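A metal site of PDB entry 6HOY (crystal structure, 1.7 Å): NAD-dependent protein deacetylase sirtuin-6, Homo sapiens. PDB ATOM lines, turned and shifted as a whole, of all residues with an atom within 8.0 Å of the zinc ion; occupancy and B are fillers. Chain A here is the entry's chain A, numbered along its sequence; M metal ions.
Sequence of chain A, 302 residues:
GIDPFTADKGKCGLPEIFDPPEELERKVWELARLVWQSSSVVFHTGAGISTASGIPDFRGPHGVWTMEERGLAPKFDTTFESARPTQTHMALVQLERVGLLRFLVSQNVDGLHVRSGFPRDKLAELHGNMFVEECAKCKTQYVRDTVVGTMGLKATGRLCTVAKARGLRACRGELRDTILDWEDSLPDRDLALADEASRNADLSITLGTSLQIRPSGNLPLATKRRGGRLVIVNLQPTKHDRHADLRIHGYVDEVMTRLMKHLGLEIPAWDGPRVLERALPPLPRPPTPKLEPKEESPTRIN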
ATOM      1  N   GLU A 134      15.008 -10.221 -19.524  1.00  0.00           N
ATOM      2  CA  GLU A 134      14.723 -11.678 -19.558  1.00  0.00           C
ATOM      3  C   GLU A 134      14.217 -12.151 -18.187  1.00  0.00           C
ATOM      4  O   GLU A 134      14.808 -11.763 -17.185  1.00  0.00           O
ATOM      5  CB  GLU A 134      16.025 -12.396 -19.901  1.00  0.00           C
ATOM      6  CG  GLU A 134      15.887 -13.901 -19.943  1.00  0.00           C
ATOM      7  CD  GLU A 134      17.229 -14.507 -20.279  1.00  0.00           C
ATOM      8  OE1 GLU A 134      17.703 -14.258 -21.413  1.00  0.00           O
ATOM      9  OE2 GLU A 134      17.834 -15.105 -19.380  1.00  0.00           O
ATOM     10  N   CYS A 135      13.089 -12.871 -18.182  1.00  0.00           N
ATOM     11  CA  CYS A 135      12.417 -13.458 -16.982  1.00  0.00           C
ATOM     12  C   CYS A 135      13.405 -14.458 -16.363  1.00  0.00           C
ATOM     13  O   CYS A 135      13.707 -15.492 -17.046  1.00  0.00           O
ATOM     14  CB  CYS A 135      11.063 -14.106 -17.331  1.00  0.00           C
ATOM     15  SG  CYS A 135      10.247 -15.044 -15.990  1.00  0.00           S
ATOM     16  N   ALA A 136      13.906 -14.155 -15.171  1.00  0.00           N
ATOM     17  CA  ALA A 136      14.729 -15.074 -14.366  1.00  0.00           C
ATOM     18  C   ALA A 136      13.990 -16.415 -14.165  1.00  0.00           C
ATOM     19  O   ALA A 136      14.682 -17.421 -13.954  1.00  0.00           O
ATOM     20  CB  ALA A 136      15.143 -14.451 -13.074  1.00  0.00           C
ATOM     21  N   LYS A 137      12.656 -16.470 -14.296  1.00  0.00           N
ATOM     22  CA  LYS A 137      11.860 -17.715 -14.115  1.00  0.00           C
ATOM     23  C   LYS A 137      11.743 -18.499 -15.420  1.00  0.00           C
ATOM     24  O   LYS A 137      12.266 -19.624 -15.454  1.00  0.00           O
ATOM     25  CB  LYS A 137      10.466 -17.437 -13.561  1.00  0.00           C
ATOM     26  CG  LYS A 137      10.421 -17.198 -12.059  1.00  0.00           C
ATOM     27  CD  LYS A 137       9.081 -17.510 -11.435  1.00  0.00           C
ATOM     28  CE  LYS A 137       9.008 -17.138  -9.973  1.00  0.00           C
ATOM     29  NZ  LYS A 137       7.673 -17.447  -9.403  1.00  0.00           N
ATOM     30  N   CYS A 138      11.063 -17.967 -16.432  1.00  0.00           N
ATOM     31  CA  CYS A 138      10.674 -18.717 -17.664  1.00  0.00           C
ATOM     32  C   CYS A 138      11.673 -18.456 -18.814  1.00  0.00           C
ATOM     33  O   CYS A 138      11.528 -19.112 -19.825  1.00  0.00           O
ATOM     34  CB  CYS A 138       9.236 -18.409 -18.099  1.00  0.00           C
ATOM     35  SG  CYS A 138       8.802 -16.655 -18.313  1.00  0.00           S
ATOM     36  N   LYS A 139      12.626 -17.518 -18.662  1.00  0.00           N
ATOM     37  CA  LYS A 139      13.665 -17.154 -19.683  1.00  0.00           C
ATOM     38  C   LYS A 139      13.090 -16.381 -20.865  1.00  0.00           C
ATOM     39  O   LYS A 139      13.883 -16.151 -21.836  1.00  0.00           O
ATOM     40  CB  LYS A 139      14.348 -18.398 -20.265  1.00  0.00           C
ATOM     41  CG  LYS A 139      14.959 -19.328 -19.224  1.00  0.00           C
ATOM     42  CD  LYS A 139      16.073 -18.724 -18.408  1.00  0.00           C
ATOM     43  CE  LYS A 139      16.162 -19.409 -17.060  1.00  0.00           C
ATOM     44  NZ  LYS A 139      17.405 -19.035 -16.337  1.00  0.00           N
ATOM     45  N   THR A 140      11.798 -16.044 -20.833  1.00  0.00           N
ATOM     46  CA  THR A 140      11.099 -15.267 -21.872  1.00  0.00           C
ATOM     47  C   THR A 140      11.728 -13.879 -21.900  1.00  0.00           C
ATOM     48  O   THR A 140      11.841 -13.244 -20.852  1.00  0.00           O
ATOM     49  CB  THR A 140       9.594 -15.128 -21.623  1.00  0.00           C
ATOM     50  OG1 THR A 140       9.015 -16.426 -21.675  1.00  0.00           O
ATOM     51  CG2 THR A 140       8.910 -14.219 -22.622  1.00  0.00           C
ATOM     52  N   GLN A 141      12.163 -13.479 -23.082  1.00  0.00           N
ATOM     53  CA  GLN A 141      12.774 -12.183 -23.389  1.00  0.00           C
ATOM     54  C   GLN A 141      11.721 -11.180 -23.846  1.00  0.00           C
ATOM     55  O   GLN A 141      10.690 -11.530 -24.476  1.00  0.00           O
ATOM     56  CB  GLN A 141      13.905 -12.422 -24.407  1.00  0.00           C
ATOM     57  CG  GLN A 141      15.156 -12.934 -23.717  1.00  0.00           C
ATOM     58  CD  GLN A 141      16.359 -13.074 -24.623  1.00  0.00           C
ATOM     59  OE1 GLN A 141      16.246 -13.058 -25.841  1.00  0.00           O
ATOM     60  NE2 GLN A 141      17.532 -13.199 -23.997  1.00  0.00           N
ATOM     61  N   TYR A 142      11.966  -9.940 -23.493  1.00  0.00           N
ATOM     62  CA  TYR A 142      11.125  -8.799 -23.866  1.00  0.00           C
ATOM     63  C   TYR A 142      12.043  -7.768 -24.533  1.00  0.00           C
ATOM     64  O   TYR A 142      13.067  -7.339 -23.889  1.00  0.00           O
ATOM     65  CB  TYR A 142      10.505  -8.165 -22.629  1.00  0.00           C
ATOM     66  CG  TYR A 142       9.537  -9.046 -21.895  1.00  0.00           C
ATOM     67  CD1 TYR A 142      10.020 -10.024 -21.056  1.00  0.00           C
ATOM     68  CD2 TYR A 142       8.165  -8.944 -22.087  1.00  0.00           C
ATOM     69  CE1 TYR A 142       9.157 -10.882 -20.392  1.00  0.00           C
ATOM     70  CE2 TYR A 142       7.287  -9.770 -21.393  1.00  0.00           C
ATOM     71  CZ  TYR A 142       7.781 -10.755 -20.572  1.00  0.00           C
ATOM     72  OH  TYR A 142       6.896 -11.568 -19.927  1.00  0.00           O
ATOM     73  N   LEU A 159       8.140  -7.298 -13.783  1.00  0.00           N
ATOM     74  CA  LEU A 159       7.784  -8.725 -13.611  1.00  0.00           C
ATOM     75  C   LEU A 159       7.267  -9.292 -14.935  1.00  0.00           C
ATOM     76  O   LEU A 159       6.744  -8.539 -15.773  1.00  0.00           O
ATOM     77  CB  LEU A 159       6.703  -8.887 -12.529  1.00  0.00           C
ATOM     78  CG  LEU A 159       7.034  -8.322 -11.152  1.00  0.00           C
ATOM     79  CD1 LEU A 159       5.872  -8.596 -10.188  1.00  0.00           C
ATOM     80  CD2 LEU A 159       8.326  -8.918 -10.609  1.00  0.00           C
ATOM     81  N   CYS A 160       7.372 -10.595 -15.074  1.00  0.00           N
ATOM     82  CA  CYS A 160       6.982 -11.347 -16.284  1.00  0.00           C
ATOM     83  C   CYS A 160       5.445 -11.366 -16.431  1.00  0.00           C
ATOM     84  O   CYS A 160       4.758 -11.478 -15.415  1.00  0.00           O
ATOM     85  CB  CYS A 160       7.493 -12.767 -16.128  1.00  0.00           C
ATOM     86  SG  CYS A 160       7.477 -13.638 -17.688  1.00  0.00           S
ATOM     87  N   THR A 161       4.953 -11.261 -17.674  1.00  0.00           N
ATOM     88  CA  THR A 161       3.502 -11.141 -18.010  1.00  0.00           C
ATOM     89  C   THR A 161       3.068 -12.325 -18.878  1.00  0.00           C
ATOM     90  O   THR A 161       1.949 -12.275 -19.481  1.00  0.00           O
ATOM     91  CB  THR A 161       3.239  -9.767 -18.644  1.00  0.00           C
ATOM     92  OG1 THR A 161       4.161  -9.615 -19.732  1.00  0.00           O
ATOM     93  CG2 THR A 161       3.395  -8.622 -17.668  1.00  0.00           C
ATOM     94  N   VAL A 162       3.902 -13.354 -18.984  1.00  0.00           N
ATOM     95  CA  VAL A 162       3.529 -14.634 -19.659  1.00  0.00           C
ATOM     96  C   VAL A 162       2.536 -15.401 -18.755  1.00  0.00           C
ATOM     97  O   VAL A 162       2.888 -15.663 -17.601  1.00  0.00           O
ATOM     98  CB  VAL A 162       4.771 -15.481 -19.995  1.00  0.00           C
ATOM     99  CG1 VAL A 162       4.387 -16.814 -20.610  1.00  0.00           C
ATOM    100  CG2 VAL A 162       5.716 -14.741 -20.906  1.00  0.00           C
ATOM    101  N   ALA A 163       1.380 -15.824 -19.277  1.00  0.00           N
ATOM    102  CA  ALA A 163       0.397 -16.714 -18.595  1.00  0.00           C
ATOM    103  C   ALA A 163       1.140 -17.779 -17.768  1.00  0.00           C
ATOM    104  O   ALA A 163       0.663 -18.936 -17.741  1.00  0.00           O
ATOM    105  CB  ALA A 163      -0.525 -17.340 -19.615  1.00  0.00           C
ATOM    106  N   CYS A 171       3.161 -15.759 -14.848  1.00  0.00           N
ATOM    107  CA  CYS A 171       4.494 -16.197 -14.347  1.00  0.00           C
ATOM    108  C   CYS A 171       5.009 -15.279 -13.224  1.00  0.00           C
ATOM    109  O   CYS A 171       5.572 -15.818 -12.245  1.00  0.00           O
ATOM    110  CB  CYS A 171       5.535 -16.240 -15.457  1.00  0.00           C
ATOM    111  SG  CYS A 171       7.204 -16.210 -14.773  1.00  0.00           S
ATOM    112  N   ARG A 172       4.941 -13.960 -13.398  1.00  0.00           N
ATOM    113  CA  ARG A 172       5.336 -12.937 -12.381  1.00  0.00           C
ATOM    114  C   ARG A 172       6.813 -13.074 -11.981  1.00  0.00           C
ATOM    115  O   ARG A 172       7.233 -12.434 -10.994  1.00  0.00           O
ATOM    116  CB  ARG A 172       4.413 -12.986 -11.159  1.00  0.00           C
ATOM    117  CG  ARG A 172       2.962 -12.656 -11.475  1.00  0.00           C
ATOM    118  CD  ARG A 172       2.079 -12.698 -10.241  1.00  0.00           C
ATOM    119  NE  ARG A 172       2.529 -11.778  -9.191  1.00  0.00           N
ATOM    120  CZ  ARG A 172       2.388 -10.454  -9.225  1.00  0.00           C
ATOM    121  NH1 ARG A 172       1.785  -9.869 -10.247  1.00  0.00           N
ATOM    122  NH2 ARG A 172       2.840  -9.732  -8.222  1.00  0.00           N
ATOM    123  N   GLY A 173       7.612 -13.809 -12.764  1.00  0.00           N
ATOM    124  CA  GLY A 173       9.063 -13.910 -12.552  1.00  0.00           C
ATOM    125  C   GLY A 173       9.713 -12.549 -12.685  1.00  0.00           C
ATOM    126  O   GLY A 173       9.123 -11.648 -13.370  1.00  0.00           O
ATOM    127  N   GLU A 174      10.874 -12.408 -12.060  1.00  0.00           N
ATOM    128  CA  GLU A 174      11.663 -11.160 -11.943  1.00  0.00           C
ATOM    129  C   GLU A 174      12.370 -10.942 -13.283  1.00  0.00           C
ATOM    130  O   GLU A 174      13.035 -11.872 -13.734  1.00  0.00           O
ATOM    131  CB  GLU A 174      12.651 -11.316 -10.794  1.00  0.00           C
ATOM    132  CG  GLU A 174      13.647 -10.180 -10.632  1.00  0.00           C
ATOM    133  CD  GLU A 174      14.653 -10.398  -9.512  1.00  0.00           C
ATOM    134  OE1 GLU A 174      14.259 -10.205  -8.345  1.00  0.00           O
ATOM    135  OE2 GLU A 174      15.819 -10.770  -9.793  1.00  0.00           O
ATOM    136  N   LEU A 175      12.138  -9.794 -13.928  1.00  0.00           N
ATOM    137  CA  LEU A 175      12.835  -9.432 -15.194  1.00  0.00           C
ATOM    138  C   LEU A 175      14.216  -8.874 -14.831  1.00  0.00           C
ATOM    139  O   LEU A 175      14.353  -8.087 -13.868  1.00  0.00           O
ATOM    140  CB  LEU A 175      11.993  -8.421 -15.981  1.00  0.00           C
ATOM    141  CG  LEU A 175      10.618  -8.941 -16.442  1.00  0.00           C
ATOM    142  CD1 LEU A 175      10.045  -8.047 -17.529  1.00  0.00           C
ATOM    143  CD2 LEU A 175      10.701 -10.392 -16.979  1.00  0.00           C
HETATM  144 ZN    ZN M   1       8.407 -15.487 -16.845  1.00  0.00          ZN
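The zinc ion is bound by the side-chain sulfur (SG) of Cys 138, 1.9 Å away. The zinc ion is bound by SG of Cys 135 (2.1 Å). SG of Cys 160 is bound to the zinc ion (2.2 Å). The zinc ion is bound by SG of Cys 171 (2.5 Å).
Four residues have an atom within 4 Å of the zinc ion: Cys 135, Cys 138, Cys 160 and Cys 171.
The side-chain hydroxyl of Thr 140 sits close to the side-chain sulfur of Cys 138, at 3.4 Å. The side-chain sulfur (SG) of Cys 135 lies close to the backbone NH (N) of Lys 137, 3.3 Å away. The backbone NH (N) of Cys 135 sits at hydrogen-bond distance from the backbone carbonyl oxygen (O) of Thr 140 (3.0 Å). N of Cys 160 sits at hydrogen-bond distance from O of Gly 173, 2.7 Å away. The backbone carbonyl oxygen (O) of Cys 160 is in hydrogen-bond range of the backbone NH (N) of Arg 172 (3.2 Å). OH of Tyr 142 lies close to SG of Cys 160, at 3.1 Å. The side-chain sulfur of Cys 171 lies close to the backbone NH of Gly 173 (3.2 Å). The backbone NH (N) of Cys 171 is in hydrogen-bond range of the backbone carbonyl oxygen (O) of Val 162 (2.8 Å).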
